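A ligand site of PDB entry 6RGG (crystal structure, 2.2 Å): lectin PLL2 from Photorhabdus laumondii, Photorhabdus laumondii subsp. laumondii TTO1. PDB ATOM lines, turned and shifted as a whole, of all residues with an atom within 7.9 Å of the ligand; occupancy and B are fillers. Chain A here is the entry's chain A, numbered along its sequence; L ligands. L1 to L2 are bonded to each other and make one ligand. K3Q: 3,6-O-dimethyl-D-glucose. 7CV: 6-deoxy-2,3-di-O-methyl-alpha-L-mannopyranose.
CA of Gly 317 touches O3 of K3Q L1 (3.3 Å).
CA of Gly 339 touches O4 of K3Q L1, 3.1 Å away.
CH2 of Trp 345 touches O1 of 7CV L2, 3.6 Å away.
CB of Trp 357 touches O2 of K3Q L1, 3.4 Å away.
Hydrophobic or aromatic side chains that line the ligand: Trp 345 and Trp 357.
An oxygen (O4) of K3Q L1 sits close to the side-chain hydroxyl of Thr 340.
N of Thr 318 lies within hydrogen-bond range of O3 of K3Q L1 (2.9 Å).
The backbone NH of Thr 340 lies within hydrogen-bond range of an oxygen (O4) of K3Q L1 (3.2 Å).
O of Thr 318 lies within hydrogen-bond range of O4 of K3Q L1 (2.7 Å).
The indole nitrogen of Trp 357 sits at hydrogen-bond distance from the backbone carbonyl oxygen of Leu 315.
N of Trp 345 sits at hydrogen-bond distance from O of Ala 337, 2.8 Å away.
O of Gly 339 lies within hydrogen-bond range of OG1 of Thr 320, 2.8 Å away.
The indole nitrogen (NE1) of Trp 345 sits at hydrogen-bond distance from the side-chain carboxylate (OD1) of Asp 341 (3.1 Å).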
ATOM      1  N   ASN A 294     -15.459 -10.846   3.544  1.00  0.00           N
ATOM      2  CA  ASN A 294     -15.942 -11.023   4.946  1.00  0.00           C
ATOM      3  C   ASN A 294     -17.446 -10.734   5.036  1.00  0.00           C
ATOM      4  O   ASN A 294     -17.968 -10.618   6.149  1.00  0.00           O
ATOM      5  CB  ASN A 294     -15.125 -10.198   5.940  1.00  0.00           C
ATOM      6  CG  ASN A 294     -13.704 -10.722   6.070  1.00  0.00           C
ATOM      7  OD1 ASN A 294     -13.470 -11.921   5.954  1.00  0.00           O
ATOM      8  ND2 ASN A 294     -12.751  -9.837   6.305  1.00  0.00           N
ATOM      9  N   ALA A 295     -18.125 -10.649   3.898  1.00  0.00           N
ATOM     10  CA  ALA A 295     -19.607 -10.585   3.828  1.00  0.00           C
ATOM     11  C   ALA A 295     -20.192 -12.010   3.883  1.00  0.00           C
ATOM     12  O   ALA A 295     -19.477 -12.986   3.569  1.00  0.00           O
ATOM     13  CB  ALA A 295     -20.036  -9.871   2.570  1.00  0.00           C
ATOM     14  N   LEU A 296     -21.469 -12.104   4.261  1.00  0.00           N
ATOM     15  CA  LEU A 296     -22.256 -13.359   4.303  1.00  0.00           C
ATOM     16  C   LEU A 296     -22.779 -13.663   2.898  1.00  0.00           C
ATOM     17  O   LEU A 296     -23.508 -12.817   2.335  1.00  0.00           O
ATOM     18  CB  LEU A 296     -23.433 -13.170   5.267  1.00  0.00           C
ATOM     19  CG  LEU A 296     -24.361 -14.377   5.400  1.00  0.00           C
ATOM     20  CD1 LEU A 296     -23.660 -15.517   6.103  1.00  0.00           C
ATOM     21  CD2 LEU A 296     -25.625 -13.993   6.143  1.00  0.00           C
ATOM     22  N   LEU A 315     -25.418 -11.370   1.131  1.00  0.00           N
ATOM     23  CA  LEU A 315     -26.353 -10.668   2.044  1.00  0.00           C
ATOM     24  C   LEU A 315     -25.623  -9.518   2.736  1.00  0.00           C
ATOM     25  O   LEU A 315     -26.228  -8.889   3.607  1.00  0.00           O
ATOM     26  CB  LEU A 315     -26.904 -11.681   3.054  1.00  0.00           C
ATOM     27  CG  LEU A 315     -27.723 -12.803   2.424  1.00  0.00           C
ATOM     28  CD1 LEU A 315     -27.974 -13.911   3.435  1.00  0.00           C
ATOM     29  CD2 LEU A 315     -29.032 -12.255   1.859  1.00  0.00           C
ATOM     30  N   ASN A 316     -24.387  -9.246   2.296  1.00  0.00           N
ATOM     31  CA  ASN A 316     -23.504  -8.134   2.744  1.00  0.00           C
ATOM     32  C   ASN A 316     -23.128  -8.360   4.217  1.00  0.00           C
ATOM     33  O   ASN A 316     -22.862  -9.526   4.580  1.00  0.00           O
ATOM     34  CB  ASN A 316     -24.131  -6.772   2.428  1.00  0.00           C
ATOM     35  CG  ASN A 316     -24.329  -6.565   0.946  1.00  0.00           C
ATOM     36  OD1 ASN A 316     -25.462  -6.448   0.486  1.00  0.00           O
ATOM     37  ND2 ASN A 316     -23.236  -6.569   0.188  1.00  0.00           N
ATOM     38  N   GLY A 317     -23.105  -7.300   5.030  1.00  0.00           N
ATOM     39  CA  GLY A 317     -22.521  -7.313   6.380  1.00  0.00           C
ATOM     40  C   GLY A 317     -21.018  -7.536   6.321  1.00  0.00           C
ATOM     41  O   GLY A 317     -20.490  -7.729   5.229  1.00  0.00           O
ATOM     42  N   THR A 318     -20.355  -7.512   7.467  1.00  0.00           N
ATOM     43  CA  THR A 318     -18.938  -7.895   7.672  1.00  0.00           C
ATOM     44  C   THR A 318     -18.906  -8.745   8.951  1.00  0.00           C
ATOM     45  O   THR A 318     -19.356  -8.226  10.012  1.00  0.00           O
ATOM     46  CB  THR A 318     -18.019  -6.658   7.777  1.00  0.00           C
ATOM     47  OG1 THR A 318     -18.130  -5.888   6.577  1.00  0.00           O
ATOM     48  CG2 THR A 318     -16.559  -7.004   7.964  1.00  0.00           C
ATOM     49  N   ILE A 319     -18.465 -10.000   8.847  1.00  0.00           N
ATOM     50  CA  ILE A 319     -18.611 -10.977   9.968  1.00  0.00           C
ATOM     51  C   ILE A 319     -17.225 -11.553  10.337  1.00  0.00           C
ATOM     52  O   ILE A 319     -16.328 -11.585   9.488  1.00  0.00           O
ATOM     53  CB  ILE A 319     -19.696 -12.031   9.647  1.00  0.00           C
ATOM     54  CG1 ILE A 319     -19.393 -12.859   8.404  1.00  0.00           C
ATOM     55  CG2 ILE A 319     -21.044 -11.337   9.523  1.00  0.00           C
ATOM     56  CD1 ILE A 319     -20.290 -14.073   8.243  1.00  0.00           C
ATOM     57  N   THR A 320     -17.087 -11.865  11.623  1.00  0.00           N
ATOM     58  CA  THR A 320     -15.852 -12.291  12.324  1.00  0.00           C
ATOM     59  C   THR A 320     -16.102 -13.673  12.936  1.00  0.00           C
ATOM     60  O   THR A 320     -15.392 -14.052  13.874  1.00  0.00           O
ATOM     61  CB  THR A 320     -15.466 -11.274  13.409  1.00  0.00           C
ATOM     62  OG1 THR A 320     -16.597 -11.131  14.281  1.00  0.00           O
ATOM     63  CG2 THR A 320     -15.082  -9.931  12.847  1.00  0.00           C
ATOM     64  N   ALA A 337     -24.429 -14.008  13.305  1.00  0.00           N
ATOM     65  CA  ALA A 337     -22.961 -13.928  13.126  1.00  0.00           C
ATOM     66  C   ALA A 337     -22.399 -12.814  13.998  1.00  0.00           C
ATOM     67  O   ALA A 337     -23.137 -11.830  14.285  1.00  0.00           O
ATOM     68  CB  ALA A 337     -22.629 -13.689  11.681  1.00  0.00           C
ATOM     69  N   ARG A 338     -21.137 -12.949  14.378  1.00  0.00           N
ATOM     70  CA  ARG A 338     -20.420 -11.895  15.117  1.00  0.00           C
ATOM     71  C   ARG A 338     -20.049 -10.815  14.092  1.00  0.00           C
ATOM     72  O   ARG A 338     -19.654 -11.209  12.979  1.00  0.00           O
ATOM     73  CB  ARG A 338     -19.185 -12.442  15.825  1.00  0.00           C
ATOM     74  CG  ARG A 338     -18.572 -11.421  16.770  1.00  0.00           C
ATOM     75  CD  ARG A 338     -17.440 -11.942  17.600  1.00  0.00           C
ATOM     76  NE  ARG A 338     -16.315 -12.387  16.789  1.00  0.00           N
ATOM     77  CZ  ARG A 338     -15.167 -12.823  17.292  1.00  0.00           C
ATOM     78  NH1 ARG A 338     -14.989 -12.881  18.607  1.00  0.00           N
ATOM     79  NH2 ARG A 338     -14.215 -13.241  16.496  1.00  0.00           N
ATOM     80  N   GLY A 339     -20.179  -9.539  14.459  1.00  0.00           N
ATOM     81  CA  GLY A 339     -19.678  -8.402  13.642  1.00  0.00           C
ATOM     82  C   GLY A 339     -18.275  -7.989  14.037  1.00  0.00           C
ATOM     83  O   GLY A 339     -17.671  -8.659  14.910  1.00  0.00           O
ATOM     84  N   THR A 340     -17.748  -6.904  13.452  1.00  0.00           N
ATOM     85  CA  THR A 340     -16.406  -6.339  13.783  1.00  0.00           C
ATOM     86  C   THR A 340     -16.426  -5.668  15.156  1.00  0.00           C
ATOM     87  O   THR A 340     -15.359  -5.645  15.803  1.00  0.00           O
ATOM     88  CB  THR A 340     -15.880  -5.430  12.660  1.00  0.00           C
ATOM     89  OG1 THR A 340     -16.984  -4.928  11.909  1.00  0.00           O
ATOM     90  CG2 THR A 340     -14.933  -6.162  11.734  1.00  0.00           C
ATOM     91  N   ASP A 341     -17.592  -5.204  15.632  1.00  0.00           N
ATOM     92  CA  ASP A 341     -17.786  -4.699  17.023  1.00  0.00           C
ATOM     93  C   ASP A 341     -17.868  -5.853  18.034  1.00  0.00           C
ATOM     94  O   ASP A 341     -18.170  -5.578  19.211  1.00  0.00           O
ATOM     95  CB  ASP A 341     -19.052  -3.849  17.126  1.00  0.00           C
ATOM     96  CG  ASP A 341     -20.337  -4.550  16.673  1.00  0.00           C
ATOM     97  OD1 ASP A 341     -20.282  -5.760  16.318  1.00  0.00           O
ATOM     98  OD2 ASP A 341     -21.383  -3.851  16.657  1.00  0.00           O
ATOM     99  N   ASN A 342     -17.690  -7.115  17.614  1.00  0.00           N
ATOM    100  CA  ASN A 342     -17.833  -8.322  18.477  1.00  0.00           C
ATOM    101  C   ASN A 342     -19.247  -8.437  19.083  1.00  0.00           C
ATOM    102  O   ASN A 342     -19.404  -9.209  20.049  1.00  0.00           O
ATOM    103  CB  ASN A 342     -16.751  -8.367  19.557  1.00  0.00           C
ATOM    104  CG  ASN A 342     -15.376  -8.603  18.956  1.00  0.00           C
ATOM    105  OD1 ASN A 342     -15.256  -9.035  17.816  1.00  0.00           O
ATOM    106  ND2 ASN A 342     -14.343  -8.320  19.729  1.00  0.00           N
ATOM    107  N   ALA A 343     -20.258  -7.770  18.511  1.00  0.00           N
ATOM    108  CA  ALA A 343     -21.676  -7.993  18.860  1.00  0.00           C
ATOM    109  C   ALA A 343     -22.256  -9.080  17.949  1.00  0.00           C
ATOM    110  O   ALA A 343     -21.628  -9.408  16.915  1.00  0.00           O
ATOM    111  CB  ALA A 343     -22.472  -6.715  18.733  1.00  0.00           C
ATOM    112  N   LEU A 344     -23.427  -9.605  18.323  1.00  0.00           N
ATOM    113  CA  LEU A 344     -24.186 -10.561  17.491  1.00  0.00           C
ATOM    114  C   LEU A 344     -25.142  -9.792  16.587  1.00  0.00           C
ATOM    115  O   LEU A 344     -25.938  -8.986  17.112  1.00  0.00           O
ATOM    116  CB  LEU A 344     -24.955 -11.545  18.375  1.00  0.00           C
ATOM    117  CG  LEU A 344     -25.561 -12.733  17.617  1.00  0.00           C
ATOM    118  CD1 LEU A 344     -24.477 -13.602  17.001  1.00  0.00           C
ATOM    119  CD2 LEU A 344     -26.450 -13.560  18.536  1.00  0.00           C
ATOM    120  N   TRP A 345     -25.076 -10.072  15.271  1.00  0.00           N
ATOM    121  CA  TRP A 345     -25.966  -9.496  14.234  1.00  0.00           C
ATOM    122  C   TRP A 345     -26.899 -10.594  13.699  1.00  0.00           C
ATOM    123  O   TRP A 345     -26.471 -11.748  13.609  1.00  0.00           O
ATOM    124  CB  TRP A 345     -25.122  -8.840  13.131  1.00  0.00           C
ATOM    125  CG  TRP A 345     -24.335  -7.660  13.610  1.00  0.00           C
ATOM    126  CD1 TRP A 345     -23.150  -7.697  14.293  1.00  0.00           C
ATOM    127  CD2 TRP A 345     -24.679  -6.271  13.497  1.00  0.00           C
ATOM    128  NE1 TRP A 345     -22.742  -6.437  14.611  1.00  0.00           N
ATOM    129  CE2 TRP A 345     -23.650  -5.533  14.126  1.00  0.00           C
ATOM    130  CE3 TRP A 345     -25.747  -5.562  12.930  1.00  0.00           C
ATOM    131  CZ2 TRP A 345     -23.651  -4.141  14.179  1.00  0.00           C
ATOM    132  CZ3 TRP A 345     -25.745  -4.191  12.990  1.00  0.00           C
ATOM    133  CH2 TRP A 345     -24.717  -3.489  13.609  1.00  0.00           C
ATOM    134  N   ASN A 346     -28.141 -10.222  13.374  1.00  0.00           N
ATOM    135  CA  ASN A 346     -29.223 -11.096  12.875  1.00  0.00           C
ATOM    136  C   ASN A 346     -29.676 -10.556  11.518  1.00  0.00           C
ATOM    137  O   ASN A 346     -29.618  -9.351  11.294  1.00  0.00           O
ATOM    138  CB  ASN A 346     -30.376 -11.120  13.886  1.00  0.00           C
ATOM    139  CG  ASN A 346     -31.709 -11.595  13.311  1.00  0.00           C
ATOM    140  OD1 ASN A 346     -32.670 -10.842  13.288  1.00  0.00           O
ATOM    141  ND2 ASN A 346     -31.766 -12.855  12.885  1.00  0.00           N
ATOM    142  N   ILE A 347     -30.082 -11.432  10.610  1.00  0.00           N
ATOM    143  CA  ILE A 347     -30.773 -11.062   9.349  1.00  0.00           C
ATOM    144  C   ILE A 347     -31.765 -12.186   9.084  1.00  0.00           C
ATOM    145  O   ILE A 347     -31.448 -13.321   9.468  1.00  0.00           O
ATOM    146  CB  ILE A 347     -29.755 -10.810   8.209  1.00  0.00           C
ATOM    147  CG1 ILE A 347     -30.407 -10.185   6.977  1.00  0.00           C
ATOM    148  CG2 ILE A 347     -28.993 -12.092   7.881  1.00  0.00           C
ATOM    149  CD1 ILE A 347     -29.420  -9.859   5.849  1.00  0.00           C
ATOM    150  N   ALA A 356     -32.844  -5.971   6.442  1.00  0.00           N
ATOM    151  CA  ALA A 356     -31.649  -5.252   6.928  1.00  0.00           C
ATOM    152  C   ALA A 356     -31.012  -6.097   8.033  1.00  0.00           C
ATOM    153  O   ALA A 356     -31.746  -6.797   8.741  1.00  0.00           O
ATOM    154  CB  ALA A 356     -32.066  -3.909   7.461  1.00  0.00           C
ATOM    155  N   TRP A 357     -29.676  -6.029   8.144  1.00  0.00           N
ATOM    156  CA  TRP A 357     -28.908  -6.499   9.313  1.00  0.00           C
ATOM    157  C   TRP A 357     -29.307  -5.683  10.557  1.00  0.00           C
ATOM    158  O   TRP A 357     -29.376  -4.444  10.429  1.00  0.00           O
ATOM    159  CB  TRP A 357     -27.415  -6.364   9.046  1.00  0.00           C
ATOM    160  CG  TRP A 357     -26.811  -7.413   8.173  1.00  0.00           C
ATOM    161  CD1 TRP A 357     -26.460  -7.282   6.859  1.00  0.00           C
ATOM    162  CD2 TRP A 357     -26.396  -8.727   8.576  1.00  0.00           C
ATOM    163  NE1 TRP A 357     -25.857  -8.432   6.422  1.00  0.00           N
ATOM    164  CE2 TRP A 357     -25.813  -9.342   7.440  1.00  0.00           C
ATOM    165  CE3 TRP A 357     -26.471  -9.450   9.775  1.00  0.00           C
ATOM    166  CZ2 TRP A 357     -25.312 -10.639   7.471  1.00  0.00           C
ATOM    167  CZ3 TRP A 357     -25.965 -10.739   9.810  1.00  0.00           C
ATOM    168  CH2 TRP A 357     -25.390 -11.318   8.673  1.00  0.00           C
ATOM    169  N   VAL A 358     -29.478  -6.349  11.700  1.00  0.00           N
ATOM    170  CA  VAL A 358     -29.778  -5.730  13.029  1.00  0.00           C
ATOM    171  C   VAL A 358     -28.835  -6.319  14.065  1.00  0.00           C
ATOM    172  O   VAL A 358     -28.548  -7.535  13.996  1.00  0.00           O
ATOM    173  CB  VAL A 358     -31.232  -5.930  13.469  1.00  0.00           C
ATOM    174  CG1 VAL A 358     -31.547  -5.143  14.721  1.00  0.00           C
ATOM    175  CG2 VAL A 358     -32.217  -5.583  12.368  1.00  0.00           C
ATOM    176  N   SER A 359     -28.415  -5.490  15.027  1.00  0.00           N
ATOM    177  CA  SER A 359     -27.555  -5.857  16.173  1.00  0.00           C
ATOM    178  C   SER A 359     -28.419  -6.308  17.339  1.00  0.00           C
ATOM    179  O   SER A 359     -29.415  -5.630  17.650  1.00  0.00           O
ATOM    180  CB  SER A 359     -26.674  -4.706  16.567  1.00  0.00           C
ATOM    181  OG  SER A 359     -25.869  -5.048  17.678  1.00  0.00           O
HETATM  182  C1  K3Q L   1     -22.742  -3.340   9.782  1.00  0.00           C
HETATM  183  C2  K3Q L   1     -22.849  -4.759   9.224  1.00  0.00           C
HETATM  184  O2  K3Q L   1     -24.234  -5.041   9.036  1.00  0.00           O
HETATM  185  O5  K3Q L   1     -21.409  -3.019  10.160  1.00  0.00           O
HETATM  186  C5  K3Q L   1     -20.928  -3.830  11.207  1.00  0.00           C
HETATM  187  C4  K3Q L   1     -20.828  -5.238  10.606  1.00  0.00           C
HETATM  188  O4  K3Q L   1     -20.193  -6.167  11.499  1.00  0.00           O
HETATM  189  C3  K3Q L   1     -22.222  -5.724  10.219  1.00  0.00           C
HETATM  190  O3  K3Q L   1     -22.181  -7.019   9.608  1.00  0.00           O
HETATM  191  C6  K3Q L   1     -19.645  -3.163  11.708  1.00  0.00           C
HETATM  192  O6  K3Q L   1     -20.024  -2.193  12.709  1.00  0.00           O
HETATM  193  C7  K3Q L   1     -23.211  -7.862  10.150  1.00  0.00           C
HETATM  194  C8  K3Q L   1     -19.107  -1.100  12.898  1.00  0.00           C
HETATM  195  C1  7CV L   2     -24.559   0.631  11.756  1.00  0.00           C
HETATM  196  C2  7CV L   2     -23.492   0.917  10.678  1.00  0.00           C
HETATM  197  C3  7CV L   2     -22.787  -0.276  10.062  1.00  0.00           C
HETATM  198  C4  7CV L   2     -23.900  -1.150   9.514  1.00  0.00           C
HETATM  199  C5  7CV L   2     -25.069  -1.360  10.496  1.00  0.00           C
HETATM  200  C6  7CV L   2     -26.249  -2.021   9.806  1.00  0.00           C
HETATM  201  O2  7CV L   2     -24.123   1.546   9.543  1.00  0.00           O
HETATM  202  O3  7CV L   2     -21.924   0.152   8.990  1.00  0.00           O
HETATM  203  O4  7CV L   2     -23.343  -2.388   9.087  1.00  0.00           O
HETATM  204  O5  7CV L   2     -25.549  -0.147  11.101  1.00  0.00           O
HETATM  205  C24 7CV L   2     -23.368   2.598   8.932  1.00  0.00           C
HETATM  206  C27 7CV L   2     -20.545  -0.256   8.962  1.00  0.00           C
HETATM  207  O1  7CV L   2     -24.129   0.047  13.036  1.00  0.00           O
